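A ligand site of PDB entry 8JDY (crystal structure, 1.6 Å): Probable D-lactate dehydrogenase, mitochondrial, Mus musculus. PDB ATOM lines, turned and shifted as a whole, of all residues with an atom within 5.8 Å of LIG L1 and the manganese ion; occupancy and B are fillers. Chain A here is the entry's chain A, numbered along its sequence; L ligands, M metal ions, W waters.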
ATOM      1  N   VAL A  88       3.753  -5.852 -31.683  1.00  0.00           N
ATOM      2  CA  VAL A  88       3.887  -7.083 -30.904  1.00  0.00           C
ATOM      3  C   VAL A  88       3.164  -8.276 -31.531  1.00  0.00           C
ATOM      4  O   VAL A  88       2.948  -9.288 -30.862  1.00  0.00           O
ATOM      5  CB  VAL A  88       3.410  -6.863 -29.453  1.00  0.00           C
ATOM      6  CG1 VAL A  88       4.291  -5.845 -28.734  1.00  0.00           C
ATOM      7  CG2 VAL A  88       1.962  -6.405 -29.416  1.00  0.00           C
ATOM      8  N   GLY A 146       2.941   2.552 -24.547  1.00  0.00           N
ATOM      9  CA  GLY A 146       4.126   2.645 -23.709  1.00  0.00           C
ATOM     10  C   GLY A 146       5.392   2.875 -24.505  1.00  0.00           C
ATOM     11  O   GLY A 146       6.348   3.463 -23.995  1.00  0.00           O
ATOM     12  N   SER A 160      -4.238   2.080 -29.033  1.00  0.00           N
ATOM     13  CA  SER A 160      -4.837   2.882 -27.973  1.00  0.00           C
ATOM     14  C   SER A 160      -3.801   3.085 -26.887  1.00  0.00           C
ATOM     15  O   SER A 160      -2.598   3.061 -27.160  1.00  0.00           O
ATOM     16  CB  SER A 160      -6.147   2.269 -27.459  1.00  0.00           C
ATOM     17  OG  SER A 160      -5.977   1.129 -26.636  1.00  0.00           O
ATOM     18  N   GLY A 161      -4.242   3.287 -25.654  1.00  0.00           N
ATOM     19  CA  GLY A 161      -3.290   3.486 -24.573  1.00  0.00           C
ATOM     20  C   GLY A 161      -4.023   3.808 -23.296  1.00  0.00           C
ATOM     21  O   GLY A 161      -5.250   3.699 -23.226  1.00  0.00           O
ATOM     22  N   GLU A 264      -5.849   2.034 -14.853  1.00  0.00           N
ATOM     23  CA  GLU A 264      -4.999   0.938 -15.281  1.00  0.00           C
ATOM     24  C   GLU A 264      -4.923  -0.100 -14.167  1.00  0.00           C
ATOM     25  O   GLU A 264      -4.707   0.252 -13.008  1.00  0.00           O
ATOM     26  CB  GLU A 264      -3.598   1.438 -15.595  1.00  0.00           C
ATOM     27  CG  GLU A 264      -3.541   2.271 -16.869  1.00  0.00           C
ATOM     28  CD  GLU A 264      -3.817   1.447 -18.109  1.00  0.00           C
ATOM     29  OE1 GLU A 264      -3.133   0.428 -18.329  1.00  0.00           O
ATOM     30  OE2 GLU A 264      -4.715   1.845 -18.892  1.00  0.00           O
ATOM     31  N   ARG A 334       4.403   2.267 -15.526  1.00  0.00           N
ATOM     32  CA  ARG A 334       3.329   1.574 -16.229  1.00  0.00           C
ATOM     33  C   ARG A 334       3.714   1.355 -17.689  1.00  0.00           C
ATOM     34  O   ARG A 334       3.585   0.248 -18.220  1.00  0.00           O
ATOM     35  CB  ARG A 334       2.025   2.370 -16.132  1.00  0.00           C
ATOM     36  CG  ARG A 334       0.935   1.927 -17.096  1.00  0.00           C
ATOM     37  CD  ARG A 334       0.523   0.490 -16.849  1.00  0.00           C
ATOM     38  NE  ARG A 334      -0.443   0.046 -17.859  1.00  0.00           N
ATOM     39  CZ  ARG A 334      -0.111  -0.529 -19.015  1.00  0.00           C
ATOM     40  NH1 ARG A 334       1.167  -0.768 -19.308  1.00  0.00           N
ATOM     41  NH2 ARG A 334      -1.062  -0.887 -19.876  1.00  0.00           N
ATOM     42  N   HIS A 335       4.226   2.411 -18.345  1.00  0.00           N
ATOM     43  CA  HIS A 335       4.539   2.306 -19.762  1.00  0.00           C
ATOM     44  C   HIS A 335       5.644   1.302 -20.034  1.00  0.00           C
ATOM     45  O   HIS A 335       5.737   0.775 -21.146  1.00  0.00           O
ATOM     46  CB  HIS A 335       4.929   3.687 -20.303  1.00  0.00           C
ATOM     47  CG  HIS A 335       3.757   4.581 -20.575  1.00  0.00           C
ATOM     48  ND1 HIS A 335       3.807   5.947 -20.431  1.00  0.00           N
ATOM     49  CD2 HIS A 335       2.490   4.292 -20.972  1.00  0.00           C
ATOM     50  CE1 HIS A 335       2.632   6.472 -20.733  1.00  0.00           C
ATOM     51  NE2 HIS A 335       1.819   5.486 -21.071  1.00  0.00           N
ATOM     52  N   ALA A 337       5.920  -1.582 -18.301  1.00  0.00           N
ATOM     53  CA  ALA A 337       5.489  -2.868 -17.749  1.00  0.00           C
ATOM     54  C   ALA A 337       5.992  -4.049 -18.587  1.00  0.00           C
ATOM     55  O   ALA A 337       6.353  -5.096 -18.044  1.00  0.00           O
ATOM     56  CB  ALA A 337       3.968  -2.907 -17.653  1.00  0.00           C
ATOM     57  N   TRP A 338       5.991  -3.905 -19.909  1.00  0.00           N
ATOM     58  CA  TRP A 338       6.518  -4.960 -20.782  1.00  0.00           C
ATOM     59  C   TRP A 338       7.937  -5.340 -20.402  1.00  0.00           C
ATOM     60  O   TRP A 338       8.258  -6.521 -20.261  1.00  0.00           O
ATOM     61  CB  TRP A 338       6.487  -4.457 -22.232  1.00  0.00           C
ATOM     62  CG  TRP A 338       7.028  -5.384 -23.294  1.00  0.00           C
ATOM     63  CD1 TRP A 338       8.145  -5.189 -24.048  1.00  0.00           C
ATOM     64  CD2 TRP A 338       6.433  -6.600 -23.780  1.00  0.00           C
ATOM     65  NE1 TRP A 338       8.297  -6.207 -24.953  1.00  0.00           N
ATOM     66  CE2 TRP A 338       7.257  -7.091 -24.813  1.00  0.00           C
ATOM     67  CE3 TRP A 338       5.294  -7.323 -23.430  1.00  0.00           C
ATOM     68  CZ2 TRP A 338       6.984  -8.273 -25.499  1.00  0.00           C
ATOM     69  CZ3 TRP A 338       5.014  -8.499 -24.120  1.00  0.00           C
ATOM     70  CH2 TRP A 338       5.858  -8.960 -25.145  1.00  0.00           C
ATOM     71  N   SER A 352       1.985 -11.304 -25.596  1.00  0.00           N
ATOM     72  CA  SER A 352       0.950 -10.548 -24.908  1.00  0.00           C
ATOM     73  C   SER A 352      -0.399 -10.841 -25.565  1.00  0.00           C
ATOM     74  O   SER A 352      -0.512 -10.874 -26.794  1.00  0.00           O
ATOM     75  CB  SER A 352       1.219  -9.057 -24.945  1.00  0.00           C
ATOM     76  OG  SER A 352       0.105  -8.330 -24.432  1.00  0.00           O
ATOM     77  N   ASP A 354      -4.560  -9.537 -25.632  1.00  0.00           N
ATOM     78  CA  ASP A 354      -5.120  -8.196 -25.817  1.00  0.00           C
ATOM     79  C   ASP A 354      -6.640  -8.235 -25.976  1.00  0.00           C
ATOM     80  O   ASP A 354      -7.212  -7.420 -26.705  1.00  0.00           O
ATOM     81  CB  ASP A 354      -4.449  -7.534 -27.030  1.00  0.00           C
ATOM     82  CG  ASP A 354      -4.883  -6.097 -27.249  1.00  0.00           C
ATOM     83  OD1 ASP A 354      -5.154  -5.376 -26.264  1.00  0.00           O
ATOM     84  OD2 ASP A 354      -4.914  -5.666 -28.426  1.00  0.00           O
ATOM     85  N   VAL A 383      -1.858  -6.787 -16.860  1.00  0.00           N
ATOM     86  CA  VAL A 383      -1.854  -5.338 -16.838  1.00  0.00           C
ATOM     87  C   VAL A 383      -2.822  -4.865 -17.914  1.00  0.00           C
ATOM     88  O   VAL A 383      -2.968  -5.520 -18.962  1.00  0.00           O
ATOM     89  CB  VAL A 383      -0.424  -4.785 -17.076  1.00  0.00           C
ATOM     90  CG1 VAL A 383       0.069  -5.101 -18.494  1.00  0.00           C
ATOM     91  CG2 VAL A 383      -0.352  -3.291 -16.808  1.00  0.00           C
ATOM     92  N   GLY A 384      -3.461  -3.739 -17.693  1.00  0.00           N
ATOM     93  CA  GLY A 384      -3.974  -3.021 -18.847  1.00  0.00           C
ATOM     94  C   GLY A 384      -5.189  -2.156 -18.631  1.00  0.00           C
ATOM     95  O   GLY A 384      -5.539  -1.765 -17.510  1.00  0.00           O
ATOM     96  N   HIS A 385      -5.806  -1.833 -19.775  1.00  0.00           N
ATOM     97  CA  HIS A 385      -6.725  -0.715 -19.945  1.00  0.00           C
ATOM     98  C   HIS A 385      -8.144  -1.172 -19.611  1.00  0.00           C
ATOM     99  O   HIS A 385      -9.030  -1.255 -20.463  1.00  0.00           O
ATOM    100  CB  HIS A 385      -6.624  -0.186 -21.364  1.00  0.00           C
ATOM    101  CG  HIS A 385      -5.219  -0.114 -21.883  1.00  0.00           C
ATOM    102  ND1 HIS A 385      -4.256   0.684 -21.308  1.00  0.00           N
ATOM    103  CD2 HIS A 385      -4.621  -0.730 -22.945  1.00  0.00           C
ATOM    104  CE1 HIS A 385      -3.122   0.541 -21.982  1.00  0.00           C
ATOM    105  NE2 HIS A 385      -3.312  -0.313 -22.965  1.00  0.00           N
ATOM    106  N   ASN A 390     -10.518  -3.997 -21.457  1.00  0.00           N
ATOM    107  CA  ASN A 390      -9.364  -4.523 -22.175  1.00  0.00           C
ATOM    108  C   ASN A 390      -8.271  -4.851 -21.160  1.00  0.00           C
ATOM    109  O   ASN A 390      -8.139  -4.165 -20.143  1.00  0.00           O
ATOM    110  CB  ASN A 390      -8.937  -3.432 -23.205  1.00  0.00           C
ATOM    111  CG  ASN A 390      -7.655  -3.750 -23.974  1.00  0.00           C
ATOM    112  OD1 ASN A 390      -6.793  -2.865 -24.095  1.00  0.00           O
ATOM    113  ND2 ASN A 390      -7.542  -4.937 -24.576  1.00  0.00           N
ATOM    114  N   HIS A 392      -4.120  -7.054 -20.854  1.00  0.00           N
ATOM    115  CA  HIS A 392      -3.022  -7.810 -21.432  1.00  0.00           C
ATOM    116  C   HIS A 392      -2.576  -8.859 -20.441  1.00  0.00           C
ATOM    117  O   HIS A 392      -2.373  -8.544 -19.261  1.00  0.00           O
ATOM    118  CB  HIS A 392      -1.822  -6.920 -21.746  1.00  0.00           C
ATOM    119  CG  HIS A 392      -2.152  -5.713 -22.563  1.00  0.00           C
ATOM    120  ND1 HIS A 392      -2.671  -5.779 -23.845  1.00  0.00           N
ATOM    121  CD2 HIS A 392      -2.015  -4.395 -22.292  1.00  0.00           C
ATOM    122  CE1 HIS A 392      -2.853  -4.562 -24.307  1.00  0.00           C
ATOM    123  NE2 HIS A 392      -2.446  -3.696 -23.393  1.00  0.00           N
ATOM    124  N   ILE A 394       0.707 -10.995 -20.019  1.00  0.00           N
ATOM    125  CA  ILE A 394       2.081 -11.061 -20.507  1.00  0.00           C
ATOM    126  C   ILE A 394       2.654 -12.399 -20.091  1.00  0.00           C
ATOM    127  O   ILE A 394       2.902 -12.641 -18.900  1.00  0.00           O
ATOM    128  CB  ILE A 394       2.937  -9.907 -19.950  1.00  0.00           C
ATOM    129  CG1 ILE A 394       2.385  -8.550 -20.376  1.00  0.00           C
ATOM    130  CG2 ILE A 394       4.396 -10.055 -20.384  1.00  0.00           C
ATOM    131  CD1 ILE A 394       3.139  -7.388 -19.775  1.00  0.00           C
ATOM    132  N   GLU A 429      -6.349  -3.453 -29.295  1.00  0.00           N
ATOM    133  CA  GLU A 429      -5.464  -2.405 -29.798  1.00  0.00           C
ATOM    134  C   GLU A 429      -4.217  -2.894 -30.552  1.00  0.00           C
ATOM    135  O   GLU A 429      -3.725  -2.191 -31.434  1.00  0.00           O
ATOM    136  CB  GLU A 429      -5.037  -1.495 -28.652  1.00  0.00           C
ATOM    137  CG  GLU A 429      -4.335  -2.276 -27.526  1.00  0.00           C
ATOM    138  CD  GLU A 429      -3.695  -1.392 -26.498  1.00  0.00           C
ATOM    139  OE1 GLU A 429      -3.993  -0.180 -26.459  1.00  0.00           O
ATOM    140  OE2 GLU A 429      -2.847  -1.917 -25.738  1.00  0.00           O
ATOM    141  N   HIS A 430      -3.669  -4.065 -30.199  1.00  0.00           N
ATOM    142  CA  HIS A 430      -2.381  -4.477 -30.762  1.00  0.00           C
ATOM    143  C   HIS A 430      -2.491  -4.889 -32.224  1.00  0.00           C
ATOM    144  O   HIS A 430      -1.519  -4.783 -32.975  1.00  0.00           O
ATOM    145  CB  HIS A 430      -1.794  -5.661 -29.993  1.00  0.00           C
ATOM    146  CG  HIS A 430      -1.286  -5.288 -28.646  1.00  0.00           C
ATOM    147  ND1 HIS A 430      -1.050  -6.219 -27.661  1.00  0.00           N
ATOM    148  CD2 HIS A 430      -0.955  -4.089 -28.116  1.00  0.00           C
ATOM    149  CE1 HIS A 430      -0.592  -5.609 -26.582  1.00  0.00           C
ATOM    150  NE2 HIS A 430      -0.522  -4.312 -26.826  1.00  0.00           N
HETATM  151  C1  LIG L   1       0.657  -2.126 -22.645  1.00  0.00           C
HETATM  152  O1  LIG L   1       1.686  -2.054 -21.912  1.00  0.00           O
HETATM  153  O2  LIG L   1      -0.360  -1.426 -22.420  1.00  0.00           O
HETATM  154  C2  LIG L   1       0.595  -3.061 -23.825  1.00  0.00           C
HETATM  155  O3  LIG L   1       0.066  -2.684 -24.818  1.00  0.00           O
HETATM  156  C3  LIG L   1       1.196  -4.446 -23.703  1.00  0.00           C
HETATM  157  C4  LIG L   1       2.383  -4.463 -24.641  1.00  0.00           C
HETATM  158  C5  LIG L   1       3.573  -3.878 -23.900  1.00  0.00           C
HETATM  159  C6  LIG L   1       2.671  -5.893 -25.030  1.00  0.00           C
HETATM  160  P1  LG2 L   2       5.793  -1.443 -36.508  1.00  0.00           P
HETATM  161  O1  LG2 L   2       6.118  -2.608 -35.646  1.00  0.00           O
HETATM  162  O2  LG2 L   2       6.865  -0.721 -37.269  1.00  0.00           O
HETATM  163  O3  LG2 L   2       4.642  -1.861 -37.527  1.00  0.00           O
HETATM  164  C1  LG2 L   2       3.394  -2.410 -37.031  1.00  0.00           C
HETATM  165  C2  LG2 L   2       2.498  -2.785 -38.191  1.00  0.00           C
HETATM  166  O4  LG2 L   2       2.023  -1.584 -38.833  1.00  0.00           O
HETATM  167  C3  LG2 L   2       3.157  -3.622 -39.283  1.00  0.00           C
HETATM  168  O5  LG2 L   2       2.203  -4.521 -39.822  1.00  0.00           O
HETATM  169  C4  LG2 L   2       3.646  -2.556 -40.259  1.00  0.00           C
HETATM  170  O6  LG2 L   2       3.779  -3.031 -41.594  1.00  0.00           O
HETATM  171  C5  LG2 L   2       2.542  -1.507 -40.151  1.00  0.00           C
HETATM  172  N1  LG2 L   2       2.976  -0.137 -40.358  1.00  0.00           N
HETATM  173  C6  LG2 L   2       3.868   0.601 -39.616  1.00  0.00           C
HETATM  174  N2  LG2 L   2       4.016   1.837 -40.037  1.00  0.00           N
HETATM  175  C7  LG2 L   2       3.128   1.930 -41.107  1.00  0.00           C
HETATM  176  C8  LG2 L   2       2.809   2.980 -41.971  1.00  0.00           C
HETATM  177  N3  LG2 L   2       3.338   4.195 -41.896  1.00  0.00           N
HETATM  178  N4  LG2 L   2       1.896   2.727 -42.948  1.00  0.00           N
HETATM  179  C9  LG2 L   2       1.352   1.515 -43.016  1.00  0.00           C
HETATM  180  N5  LG2 L   2       1.578   0.446 -42.241  1.00  0.00           N
HETATM  181  C10 LG2 L   2       2.486   0.719 -41.300  1.00  0.00           C
HETATM  182  N6  LG2 L   2       0.215  -0.668 -28.629  1.00  0.00           N
HETATM  183  C11 LG2 L   2      -0.988  -0.147 -28.260  1.00  0.00           C
HETATM  184  O7  LG2 L   2      -1.933  -0.069 -29.072  1.00  0.00           O
HETATM  185  N7  LG2 L   2      -1.154   0.325 -26.972  1.00  0.00           N
HETATM  186  C12 LG2 L   2      -0.209   0.310 -25.965  1.00  0.00           C
HETATM  187  O8  LG2 L   2      -0.483   0.727 -24.841  1.00  0.00           O
HETATM  188  C13 LG2 L   2       1.075  -0.226 -26.376  1.00  0.00           C
HETATM  189  N8  LG2 L   2       2.056  -0.258 -25.484  1.00  0.00           N
HETATM  190  C14 LG2 L   2       3.275  -0.781 -25.885  1.00  0.00           C
HETATM  191  C15 LG2 L   2       4.318  -0.818 -24.961  1.00  0.00           C
HETATM  192  C16 LG2 L   2       5.561  -1.339 -25.303  1.00  0.00           C
HETATM  193  C17 LG2 L   2       6.662  -1.377 -24.281  1.00  0.00           C
HETATM  194  C18 LG2 L   2       5.771  -1.831 -26.598  1.00  0.00           C
HETATM  195  C19 LG2 L   2       7.106  -2.393 -27.012  1.00  0.00           C
HETATM  196  C20 LG2 L   2       4.735  -1.788 -27.525  1.00  0.00           C
HETATM  197  C21 LG2 L   2       3.491  -1.267 -27.183  1.00  0.00           C
HETATM  198  N9  LG2 L   2       2.425  -1.190 -28.109  1.00  0.00           N
HETATM  199  C22 LG2 L   2       1.202  -0.688 -27.731  1.00  0.00           C
HETATM  200  C23 LG2 L   2       2.565  -1.773 -29.462  1.00  0.00           C
HETATM  201  C24 LG2 L   2       3.127  -0.824 -30.515  1.00  0.00           C
HETATM  202  O9  LG2 L   2       3.893   0.209 -29.896  1.00  0.00           O
HETATM  203  C25 LG2 L   2       1.981  -0.234 -31.327  1.00  0.00           C
HETATM  204  O10 LG2 L   2       1.327  -1.315 -31.989  1.00  0.00           O
HETATM  205  C26 LG2 L   2       2.447   0.784 -32.358  1.00  0.00           C
HETATM  206  O11 LG2 L   2       1.294   1.390 -32.960  1.00  0.00           O
HETATM  207  C27 LG2 L   2       3.328   0.171 -33.420  1.00  0.00           C
HETATM  208  O12 LG2 L   2       3.946   1.230 -34.184  1.00  0.00           O
HETATM  209  P2  LG2 L   2       5.309   0.985 -34.940  1.00  0.00           P
HETATM  210  O13 LG2 L   2       5.607   2.080 -35.961  1.00  0.00           O
HETATM  211  O14 LG2 L   2       6.428   0.754 -33.956  1.00  0.00           O
HETATM  212  O15 LG2 L   2       4.963  -0.376 -35.680  1.00  0.00           O
HETATM  213 MN    MN M   1      -1.751  -1.529 -24.035  1.00  0.00          MN
HETATM  214  O   HOH W   1       4.527  -1.901 -21.309  1.00  0.00           O
HETATM  215  O   HOH W   2       1.960   1.083 -22.098  1.00  0.00           O
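The side-chain carboxylate of Glu 429 sits at hydrogen-bond distance from a nitrogen (N7) of LG2 L2, 2.9 Å away.
N8 of LG2 L2 is in hydrogen-bond range of N of Gly 146, 3.1 Å away.
The backbone carbonyl oxygen (O) of Ser 160 lies within hydrogen-bond range of a nitrogen (N7) of LG2 L2, 3.1 Å away.
NH1 of Arg 334 lies within salt-bridge range of O1 of LIG L1 (3.0 Å).
O3 of LIG L1 sits close to NE2 of His 430 (2.7 Å).
An oxygen (O7) of LG2 L2 sits at hydrogen-bond distance from the backbone NH (N) of Ser 160 (3.2 Å).
The backbone NH (N) of His 392 lies within hydrogen-bond range of the backbone carbonyl oxygen (O) of Val 383, 2.7 Å away.
The backbone carbonyl oxygen of His 385 lies within hydrogen-bond range of the backbone NH of Asn 390 (3.3 Å).
NE of Arg 334 is in salt-bridge range of OE1 of Glu 264 (2.8 Å).
The side-chain carboxylate (OE2) of Glu 264 lies within hydrogen-bond range of a ring nitrogen (ND1) of His 385 (2.7 Å).
OE1 of Glu 429 sits close to N of Ser 160.
OD2 of Asp 354 lies within hydrogen-bond range of N of His 430 (2.7 Å).
The backbone NH (N) of Glu 429 sits at hydrogen-bond distance from the side-chain carboxylate (OD2) of Asp 354, 2.8 Å away.
The side-chain carboxylate (OD1) of Asp 354 lies close to a ring nitrogen (ND1) of His 392 (3.5 Å).
Trp 338 touches LIG L1 (CE3 to C6, 3.4 Å).
CB of Ser 352 touches C6 of LIG L1, at 3.5 Å.
Hydrophobic or aromatic side chains within 4 Å of LIG L1: Trp 338, His 385, His 392 and His 430.
Within 4 Å of LIG L1: Arg 334, Trp 338, Ser 352, His 385, His 392, Glu 429 and His 430.
Water W1 lies within hydrogen-bond range of the backbone NH (N) of Trp 338 (2.8 Å), an oxygen (O1) of LIG L1 (2.9 Å), the backbone carbonyl oxygen (O) of His 335 (2.9 Å) and the backbone NH (N) of Ala 337 (3.3 Å).
Water W2 lies within hydrogen-bond range of the backbone NH (N) of Gly 146, an oxygen (O1) of LIG L1 and the guanidinium group (NH1) of Arg 334.
The manganese ion is bound by the side-chain carboxylate (OE2) of Glu 429 (2.1 Å), an oxygen (O2) of LIG L1 (2.1 Å), a ring nitrogen (NE2) of His 385 (2.2 Å), an oxygen (O3) of LIG L1 (2.3 Å) and a ring nitrogen (NE2) of His 392 (2.4 Å).
The manganese ion has five donor atoms within binding distance.
Slightly farther from the manganese ion lies O8 of LG2 L2 (2.7 Å).
The nearest printed residue that does not touch the manganese ion is His 430 (4.1 Å).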
